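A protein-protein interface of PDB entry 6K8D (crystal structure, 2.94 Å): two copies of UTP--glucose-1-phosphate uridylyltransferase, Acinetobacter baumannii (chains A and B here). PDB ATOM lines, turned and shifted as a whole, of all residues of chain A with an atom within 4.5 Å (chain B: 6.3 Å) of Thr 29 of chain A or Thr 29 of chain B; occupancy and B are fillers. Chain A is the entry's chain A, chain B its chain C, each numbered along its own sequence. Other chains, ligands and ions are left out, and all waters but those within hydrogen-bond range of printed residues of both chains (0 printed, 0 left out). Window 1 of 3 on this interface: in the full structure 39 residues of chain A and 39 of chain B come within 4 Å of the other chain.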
ATOM      1  N   ALA A  19     -22.900  27.885  30.083  1.00  0.00           N
ATOM      2  CA  ALA A  19     -22.264  26.550  30.238  1.00  0.00           C
ATOM      3  C   ALA A  19     -22.869  25.810  31.427  1.00  0.00           C
ATOM      4  O   ALA A  19     -23.368  24.686  31.236  1.00  0.00           O
ATOM      5  CB  ALA A  19     -20.780  26.705  30.446  1.00  0.00           C
ATOM      6  N   ILE A  23     -25.776  21.924  34.091  1.00  0.00           N
ATOM      7  CA  ILE A  23     -24.775  21.080  34.819  1.00  0.00           C
ATOM      8  C   ILE A  23     -24.002  21.993  35.766  1.00  0.00           C
ATOM      9  O   ILE A  23     -23.882  23.175  35.487  1.00  0.00           O
ATOM     10  CB  ILE A  23     -23.820  20.355  33.846  1.00  0.00           C
ATOM     11  CG1 ILE A  23     -22.754  21.299  33.295  1.00  0.00           C
ATOM     12  CG2 ILE A  23     -24.577  19.674  32.725  1.00  0.00           C
ATOM     13  CD1 ILE A  23     -21.728  20.620  32.440  1.00  0.00           C
ATOM     14  N   MET A  27     -18.134  20.919  37.143  1.00  0.00           N
ATOM     15  CA  MET A  27     -18.154  19.708  36.282  1.00  0.00           C
ATOM     16  C   MET A  27     -17.788  20.052  34.830  1.00  0.00           C
ATOM     17  O   MET A  27     -17.719  19.116  34.001  1.00  0.00           O
ATOM     18  CB  MET A  27     -19.543  19.057  36.324  1.00  0.00           C
ATOM     19  CG  MET A  27     -19.786  18.167  37.546  1.00  0.00           C
ATOM     20  SD  MET A  27     -18.669  16.719  37.691  1.00  0.00           S
ATOM     21  CE  MET A  27     -18.812  15.964  36.072  1.00  0.00           C
ATOM     22  N   VAL A  28     -17.555  21.325  34.508  1.00  0.00           N
ATOM     23  CA  VAL A  28     -17.251  21.748  33.106  1.00  0.00           C
ATOM     24  C   VAL A  28     -15.878  21.194  32.723  1.00  0.00           C
ATOM     25  O   VAL A  28     -15.009  21.061  33.615  1.00  0.00           O
ATOM     26  CB  VAL A  28     -17.311  23.270  32.897  1.00  0.00           C
ATOM     27  CG1 VAL A  28     -18.706  23.806  33.177  1.00  0.00           C
ATOM     28  CG2 VAL A  28     -16.250  24.004  33.710  1.00  0.00           C
ATOM     29  N   THR A  29     -15.710  20.928  31.427  1.00  0.00           N
ATOM     30  CA  THR A  29     -14.681  20.027  30.856  1.00  0.00           C
ATOM     31  C   THR A  29     -13.427  20.840  30.528  1.00  0.00           C
ATOM     32  O   THR A  29     -13.475  21.706  29.625  1.00  0.00           O
ATOM     33  CB  THR A  29     -15.285  19.230  29.691  1.00  0.00           C
ATOM     34  OG1 THR A  29     -16.321  20.003  29.079  1.00  0.00           O
ATOM     35  CG2 THR A  29     -15.878  17.913  30.144  1.00  0.00           C
ATOM     36  N   VAL A  30     -12.359  20.568  31.282  1.00  0.00           N
ATOM     37  CA  VAL A  30     -10.982  21.110  31.099  1.00  0.00           C
ATOM     38  C   VAL A  30     -10.139  20.060  30.366  1.00  0.00           C
ATOM     39  O   VAL A  30      -9.602  19.157  31.040  1.00  0.00           O
ATOM     40  CB  VAL A  30     -10.367  21.483  32.454  1.00  0.00           C
ATOM     41  CG1 VAL A  30      -8.964  22.039  32.295  1.00  0.00           C
ATOM     42  CG2 VAL A  30     -11.255  22.457  33.209  1.00  0.00           C
ATOM     43  N   VAL A  31     -10.055  20.192  29.038  1.00  0.00           N
ATOM     44  CA  VAL A  31      -9.382  19.263  28.082  1.00  0.00           C
ATOM     45  C   VAL A  31     -10.248  18.010  27.898  1.00  0.00           C
ATOM     46  O   VAL A  31     -10.673  17.774  26.759  1.00  0.00           O
ATOM     47  CB  VAL A  31      -7.943  18.891  28.499  1.00  0.00           C
ATOM     48  CG1 VAL A  31      -7.182  18.236  27.347  1.00  0.00           C
ATOM     49  CG2 VAL A  31      -7.155  20.074  29.034  1.00  0.00           C
ATOM     50  N   ARG A  33     -11.584  16.135  31.251  1.00  0.00           N
ATOM     51  CA  ARG A  33     -12.020  15.711  32.602  1.00  0.00           C
ATOM     52  C   ARG A  33     -12.589  16.928  33.318  1.00  0.00           C
ATOM     53  O   ARG A  33     -12.088  18.032  33.127  1.00  0.00           O
ATOM     54  CB  ARG A  33     -10.823  15.115  33.338  1.00  0.00           C
ATOM     55  CG  ARG A  33      -9.731  16.138  33.624  1.00  0.00           C
ATOM     56  CD  ARG A  33      -8.381  15.584  34.032  1.00  0.00           C
ATOM     57  NE  ARG A  33      -8.453  14.233  34.561  1.00  0.00           N
ATOM     58  CZ  ARG A  33      -8.295  13.129  33.839  1.00  0.00           C
ATOM     59  NH1 ARG A  33      -8.385  11.952  34.436  1.00  0.00           N
ATOM     60  NH2 ARG A  33      -8.065  13.195  32.533  1.00  0.00           N
ATOM     61  N   TYR A 264     -10.807  30.279  32.683  1.00  0.00           N
ATOM     62  CA  TYR A 264     -11.075  28.868  32.291  1.00  0.00           C
ATOM     63  C   TYR A 264     -10.337  28.558  30.980  1.00  0.00           C
ATOM     64  O   TYR A 264      -9.530  27.594  30.961  1.00  0.00           O
ATOM     65  CB  TYR A 264     -12.585  28.602  32.208  1.00  0.00           C
ATOM     66  CG  TYR A 264     -13.017  27.459  31.320  1.00  0.00           C
ATOM     67  CD1 TYR A 264     -13.297  27.667  29.980  1.00  0.00           C
ATOM     68  CD2 TYR A 264     -13.193  26.172  31.814  1.00  0.00           C
ATOM     69  CE1 TYR A 264     -13.712  26.630  29.155  1.00  0.00           C
ATOM     70  CE2 TYR A 264     -13.598  25.123  30.998  1.00  0.00           C
ATOM     71  CZ  TYR A 264     -13.864  25.351  29.659  1.00  0.00           C
ATOM     72  OH  TYR A 264     -14.256  24.352  28.813  1.00  0.00           O
ATOM     73  N   PHE B  16     -15.784   9.907  24.554  1.00  0.00           N
ATOM     74  CA  PHE B  16     -15.266  11.066  25.332  1.00  0.00           C
ATOM     75  C   PHE B  16     -15.450  10.835  26.835  1.00  0.00           C
ATOM     76  O   PHE B  16     -16.520  11.170  27.362  1.00  0.00           O
ATOM     77  CB  PHE B  16     -15.905  12.400  24.930  1.00  0.00           C
ATOM     78  CG  PHE B  16     -15.028  13.606  25.200  1.00  0.00           C
ATOM     79  CD1 PHE B  16     -13.821  13.489  25.888  1.00  0.00           C
ATOM     80  CD2 PHE B  16     -15.411  14.865  24.772  1.00  0.00           C
ATOM     81  CE1 PHE B  16     -13.021  14.594  26.125  1.00  0.00           C
ATOM     82  CE2 PHE B  16     -14.615  15.971  25.021  1.00  0.00           C
ATOM     83  CZ  PHE B  16     -13.421  15.835  25.693  1.00  0.00           C
ATOM     84  N   PRO B  18     -12.913  10.701  30.751  1.00  0.00           N
ATOM     85  CA  PRO B  18     -14.029  10.784  31.688  1.00  0.00           C
ATOM     86  C   PRO B  18     -14.838  12.095  31.633  1.00  0.00           C
ATOM     87  O   PRO B  18     -15.588  12.360  32.575  1.00  0.00           O
ATOM     88  CB  PRO B  18     -13.284  10.656  33.025  1.00  0.00           C
ATOM     89  CG  PRO B  18     -11.992  11.408  32.799  1.00  0.00           C
ATOM     90  CD  PRO B  18     -11.655  11.171  31.339  1.00  0.00           C
ATOM     91  N   ALA B  19     -14.707  12.872  30.548  1.00  0.00           N
ATOM     92  CA  ALA B  19     -15.583  14.029  30.234  1.00  0.00           C
ATOM     93  C   ALA B  19     -17.040  13.699  30.604  1.00  0.00           C
ATOM     94  O   ALA B  19     -17.613  14.353  31.513  1.00  0.00           O
ATOM     95  CB  ALA B  19     -15.462  14.396  28.773  1.00  0.00           C
ATOM     96  N   SER B  20     -17.597  12.672  29.964  1.00  0.00           N
ATOM     97  CA  SER B  20     -19.040  12.351  30.001  1.00  0.00           C
ATOM     98  C   SER B  20     -19.368  11.355  31.126  1.00  0.00           C
ATOM     99  O   SER B  20     -20.508  10.829  31.160  1.00  0.00           O
ATOM    100  CB  SER B  20     -19.477  11.834  28.666  1.00  0.00           C
ATOM    101  OG  SER B  20     -19.326  10.420  28.612  1.00  0.00           O
ATOM    102  N   ILE B  23     -21.950  13.569  33.133  1.00  0.00           N
ATOM    103  CA  ILE B  23     -22.709  14.596  32.363  1.00  0.00           C
ATOM    104  C   ILE B  23     -22.816  14.065  30.945  1.00  0.00           C
ATOM    105  O   ILE B  23     -21.931  13.339  30.518  1.00  0.00           O
ATOM    106  CB  ILE B  23     -22.003  15.963  32.434  1.00  0.00           C
ATOM    107  CG1 ILE B  23     -20.658  15.974  31.699  1.00  0.00           C
ATOM    108  CG2 ILE B  23     -21.854  16.389  33.886  1.00  0.00           C
ATOM    109  CD1 ILE B  23     -19.901  17.293  31.775  1.00  0.00           C
ATOM    110  N   LYS B  25     -22.343  13.530  27.018  1.00  0.00           N
ATOM    111  CA  LYS B  25     -21.361  13.958  25.983  1.00  0.00           C
ATOM    112  C   LYS B  25     -21.893  15.228  25.291  1.00  0.00           C
ATOM    113  O   LYS B  25     -21.072  16.076  24.866  1.00  0.00           O
ATOM    114  CB  LYS B  25     -21.109  12.828  24.978  1.00  0.00           C
ATOM    115  CG  LYS B  25     -22.289  12.472  24.075  1.00  0.00           C
ATOM    116  CD  LYS B  25     -22.221  11.063  23.464  1.00  0.00           C
ATOM    117  CE  LYS B  25     -23.040  10.870  22.199  1.00  0.00           C
ATOM    118  NZ  LYS B  25     -22.388  11.488  21.015  1.00  0.00           N
ATOM    119  N   MET B  27     -23.478  17.736  26.674  1.00  0.00           N
ATOM    120  CA  MET B  27     -23.366  18.924  27.566  1.00  0.00           C
ATOM    121  C   MET B  27     -21.893  19.201  27.882  1.00  0.00           C
ATOM    122  O   MET B  27     -21.636  20.018  28.784  1.00  0.00           O
ATOM    123  CB  MET B  27     -24.124  18.709  28.879  1.00  0.00           C
ATOM    124  CG  MET B  27     -25.630  18.486  28.714  1.00  0.00           C
ATOM    125  SD  MET B  27     -26.587  19.937  28.181  1.00  0.00           S
ATOM    126  CE  MET B  27     -25.933  21.204  29.270  1.00  0.00           C
ATOM    127  N   VAL B  28     -20.965  18.548  27.173  1.00  0.00           N
ATOM    128  CA  VAL B  28     -19.503  18.872  27.165  1.00  0.00           C
ATOM    129  C   VAL B  28     -19.344  20.327  26.723  1.00  0.00           C
ATOM    130  O   VAL B  28     -19.807  20.634  25.619  1.00  0.00           O
ATOM    131  CB  VAL B  28     -18.721  17.935  26.228  1.00  0.00           C
ATOM    132  CG1 VAL B  28     -17.934  16.908  27.019  1.00  0.00           C
ATOM    133  N   THR B  29     -18.723  21.181  27.543  1.00  0.00           N
ATOM    134  CA  THR B  29     -18.743  22.654  27.345  1.00  0.00           C
ATOM    135  C   THR B  29     -17.643  23.047  26.357  1.00  0.00           C
ATOM    136  O   THR B  29     -16.462  22.837  26.664  1.00  0.00           O
ATOM    137  CB  THR B  29     -18.712  23.401  28.683  1.00  0.00           C
ATOM    138  OG1 THR B  29     -17.502  23.068  29.356  1.00  0.00           O
ATOM    139  CG2 THR B  29     -19.906  23.057  29.552  1.00  0.00           C
ATOM    140  N   VAL B  30     -18.064  23.575  25.202  1.00  0.00           N
ATOM    141  CA  VAL B  30     -17.221  24.169  24.122  1.00  0.00           C
ATOM    142  C   VAL B  30     -17.150  25.678  24.358  1.00  0.00           C
ATOM    143  O   VAL B  30     -18.200  26.340  24.219  1.00  0.00           O
ATOM    144  CB  VAL B  30     -17.797  23.897  22.718  1.00  0.00           C
ATOM    145  CG1 VAL B  30     -16.767  24.192  21.637  1.00  0.00           C
ATOM    146  CG2 VAL B  30     -18.349  22.487  22.560  1.00  0.00           C
ATOM    147  N   VAL B  31     -15.961  26.192  24.687  1.00  0.00           N
ATOM    148  CA  VAL B  31     -15.703  27.630  25.010  1.00  0.00           C
ATOM    149  C   VAL B  31     -16.457  27.984  26.297  1.00  0.00           C
ATOM    150  O   VAL B  31     -15.787  28.133  27.335  1.00  0.00           O
ATOM    151  CB  VAL B  31     -16.092  28.602  23.873  1.00  0.00           C
ATOM    152  CG1 VAL B  31     -15.467  29.969  24.098  1.00  0.00           C
ATOM    153  CG2 VAL B  31     -15.738  28.087  22.484  1.00  0.00           C
ATOM    154  N   ASP B  32     -17.789  28.118  26.223  1.00  0.00           N
ATOM    155  CA  ASP B  32     -18.625  28.673  27.323  1.00  0.00           C
ATOM    156  C   ASP B  32     -20.073  28.177  27.252  1.00  0.00           C
ATOM    157  O   ASP B  32     -20.929  28.869  27.807  1.00  0.00           O
ATOM    158  CB  ASP B  32     -18.621  30.207  27.291  1.00  0.00           C
ATOM    159  CG  ASP B  32     -19.287  30.828  26.066  1.00  0.00           C
ATOM    160  OD1 ASP B  32     -19.629  30.086  25.126  1.00  0.00           O
ATOM    161  OD2 ASP B  32     -19.461  32.059  26.062  1.00  0.00           O
ATOM    162  N   ARG B  33     -20.350  27.028  26.633  1.00  0.00           N
ATOM    163  CA  ARG B  33     -21.749  26.575  26.404  1.00  0.00           C
ATOM    164  C   ARG B  33     -21.748  25.130  25.930  1.00  0.00           C
ATOM    165  O   ARG B  33     -20.822  24.703  25.255  1.00  0.00           O
ATOM    166  CB  ARG B  33     -22.424  27.481  25.372  1.00  0.00           C
ATOM    167  CG  ARG B  33     -21.660  27.573  24.059  1.00  0.00           C
ATOM    168  CD  ARG B  33     -21.614  28.958  23.436  1.00  0.00           C
ATOM    169  NE  ARG B  33     -22.893  29.655  23.493  1.00  0.00           N
ATOM    170  CZ  ARG B  33     -23.150  30.752  24.199  1.00  0.00           C
ATOM    171  NH1 ARG B  33     -24.366  31.267  24.163  1.00  0.00           N
ATOM    172  NH2 ARG B  33     -22.220  31.335  24.934  1.00  0.00           N
ATOM    173  N   PRO B  34     -22.803  24.348  26.224  1.00  0.00           N
ATOM    174  CA  PRO B  34     -22.811  22.926  25.904  1.00  0.00           C
ATOM    175  C   PRO B  34     -22.860  22.655  24.393  1.00  0.00           C
ATOM    176  O   PRO B  34     -23.496  23.402  23.664  1.00  0.00           O
ATOM    177  CB  PRO B  34     -24.082  22.412  26.592  1.00  0.00           C
ATOM    178  CG  PRO B  34     -24.996  23.616  26.638  1.00  0.00           C
ATOM    179  CD  PRO B  34     -24.066  24.798  26.818  1.00  0.00           C
ATOM    180  N   ALA B  35     -22.189  21.587  23.970  1.00  0.00           N
ATOM    181  CA  ALA B  35     -22.032  21.184  22.560  1.00  0.00           C
ATOM    182  C   ALA B  35     -23.404  21.134  21.882  1.00  0.00           C
ATOM    183  O   ALA B  35     -23.533  21.736  20.800  1.00  0.00           O
ATOM    184  CB  ALA B  35     -21.318  19.861  22.497  1.00  0.00           C
ATOM    185  N   TYR B  38     -24.989  24.349  19.979  1.00  0.00           N
ATOM    186  CA  TYR B  38     -24.434  24.598  18.621  1.00  0.00           C
ATOM    187  C   TYR B  38     -25.206  23.818  17.550  1.00  0.00           C
ATOM    188  O   TYR B  38     -25.583  24.399  16.516  1.00  0.00           O
ATOM    189  CB  TYR B  38     -22.974  24.154  18.563  1.00  0.00           C
ATOM    190  CG  TYR B  38     -22.043  24.964  19.417  1.00  0.00           C
ATOM    191  CD1 TYR B  38     -21.512  26.144  18.939  1.00  0.00           C
ATOM    192  CD2 TYR B  38     -21.679  24.552  20.686  1.00  0.00           C
ATOM    193  CE1 TYR B  38     -20.637  26.901  19.695  1.00  0.00           C
ATOM    194  CE2 TYR B  38     -20.806  25.297  21.459  1.00  0.00           C
ATOM    195  CZ  TYR B  38     -20.282  26.479  20.962  1.00  0.00           C
ATOM    196  OH  TYR B  38     -19.412  27.251  21.683  1.00  0.00           O
ATOM    197  N   TYR B 264     -12.934  17.825  19.720  1.00  0.00           N
ATOM    198  CA  TYR B 264     -13.298  18.724  20.848  1.00  0.00           C
ATOM    199  C   TYR B 264     -12.279  19.862  20.893  1.00  0.00           C
ATOM    200  O   TYR B 264     -12.645  20.976  20.499  1.00  0.00           O
ATOM    201  CB  TYR B 264     -13.404  17.957  22.171  1.00  0.00           C
ATOM    202  CG  TYR B 264     -13.633  18.807  23.399  1.00  0.00           C
ATOM    203  CD1 TYR B 264     -14.893  19.285  23.742  1.00  0.00           C
ATOM    204  CD2 TYR B 264     -12.579  19.121  24.239  1.00  0.00           C
ATOM    205  CE1 TYR B 264     -15.095  20.061  24.876  1.00  0.00           C
ATOM    206  CE2 TYR B 264     -12.766  19.889  25.379  1.00  0.00           C
ATOM    207  CZ  TYR B 264     -14.024  20.362  25.702  1.00  0.00           C
ATOM    208  OH  TYR B 264     -14.150  21.132  26.823  1.00  0.00           O
ATOM    209  N   VAL B 268     -13.075  23.918  20.412  1.00  0.00           N
ATOM    210  CA  VAL B 268     -12.839  24.870  21.547  1.00  0.00           C
ATOM    211  C   VAL B 268     -11.791  25.923  21.143  1.00  0.00           C
ATOM    212  O   VAL B 268     -11.760  26.996  21.790  1.00  0.00           O
ATOM    213  CB  VAL B 268     -12.431  24.118  22.833  1.00  0.00           C
ATOM    214  CG1 VAL B 268     -11.903  25.044  23.924  1.00  0.00           C
ATOM    215  CG2 VAL B 268     -13.580  23.270  23.363  1.00  0.00           C
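Printed residues of chain B within 4 Å of Ala 19 of chain A: Thr 29, Asp 32 and Arg 33.
Of the printed residues of chain B, Ile 23 of chain A touches Ile 23 and Met 27.
Thr 29 of chain A touches four residues of chain B.
Of the printed residues of chain A, Ile 23 of chain B touches Ile 23 and Met 27.
Printed residues of chain A within 4 Å of Met 27 of chain B: Ile 23.
Of chain A, only Ala 19, Val 28, Thr 29 and Tyr 264 come within 4 Å of Thr 29 of chain B.
Printed residues of chain A within 4 Å of Arg 33 of chain B: Ala 19.
Tyr 38 of chain B touches none of the printed residues of chain A.
Val 268 of chain B touches none of the printed residues of chain A.
The nearest residue of chain B that does not touch Thr 29 of chain A is Ile 23 of chain B (4.4 Å).
The nearest residue of chain A that does not touch Thr 29 of chain B is Ile 23 of chain A (4.2 Å).
N of Ala 19 of chain A is in hydrogen-bond range of O of Asp 32 of chain B (3.2 Å).
N of Thr 29 of chain B lies within hydrogen-bond range of OG1 of Thr 29 of chain A (3.1 Å).
The backbone carbonyl oxygen (O) of Thr 29 of chain A sits at hydrogen-bond distance from the side-chain hydroxyl (OH) of Tyr 264 of chain B.
The backbone carbonyl oxygen (O) of Thr 29 of chain B sits at hydrogen-bond distance from the side-chain hydroxyl (OH) of Tyr 264 of chain A (3.4 Å).
Ala 19 of chain A touches Arg 33 of chain B, but with the chains exchanged Arg 33 of chain A does not touch Ala 19 of chain B (4.4 Å).
Ile 23 of chain A touches Met 27 of chain B, and with the chains exchanged Met 27 of chain A touches Ile 23 of chain B.
Thr 29 of chain B touches its own counterpart, Thr 29 of chain A.
Thr 29 of chain A touches Tyr 264 of chain B, and with the chains exchanged Tyr 264 of chain A touches Thr 29 of chain B.
Of the 17 pairs that touch across the chains among the printed residues, 13 have their exchanged pair printed and touching as well.
The backbone carbonyl oxygen (O) of Thr 29 of chain A is in hydrogen-bond range of the side-chain hydroxyl (OH) of Tyr 264 of chain A (2.9 Å).
OG of Ser 20 of chain B lies within hydrogen-bond range of O of Phe 16 of chain B, at 3.2 Å.
The backbone carbonyl oxygen of Val 28 of chain B is in hydrogen-bond range of the backbone NH of Ala 35 of chain B (3.0 Å).
OH of Tyr 264 of chain B is in hydrogen-bond range of O of Thr 29 of chain B, 2.9 Å away.
The guanidinium group (NH2) of Arg 33 of chain B lies within salt-bridge range of the side-chain carboxylate (OD1) of Asp 32 of chain B (2.9 Å).
Among the printed residues, pairs that only touch across the chains: Ala 19 of chain A with Thr 29 of chain B (3.9 Å), Ala 19 of chain A with Arg 33 of chain B (3.9 Å), Ile 23 of chain A with Ile 23 of chain B (3.9 Å), Ile 23 of chain A with Met 27 of chain B (3.7 Å), Met 27 of chain A with Ile 23 of chain B (3.6 Å), Val 28 of chain A with Thr 29 of chain B (3.6 Å), Thr 29 of chain A with Ala 19 of chain B (3.8 Å), Thr 29 of chain A with Val 28 of chain B (3.8 Å), Val 31 of chain A with Phe 16 of chain B (3.5 Å), Val 31 of chain A with Tyr 264 of chain B (3.3 Å), Arg 33 of chain A with Pro 18 of chain B (3.9 Å), Tyr 264 of chain A with Val 31 of chain B (3.1 Å) and Tyr 264 of chain A with Tyr 264 of chain B (3.8 Å).
Of the 18 printed residues of chain B, 11 touch a printed residue of chain A.
Along chain B the printed residues that touch a printed residue of chain A span positions 16 to 264.
Of the 9 printed residues of chain A, 8 touch a printed residue of chain B.
Hydrophobic or aromatic side chains of chain A within 4 Å of the printed part of chain B: Ala 19, Ile 23, Met 27, Val 28 and Tyr 264.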
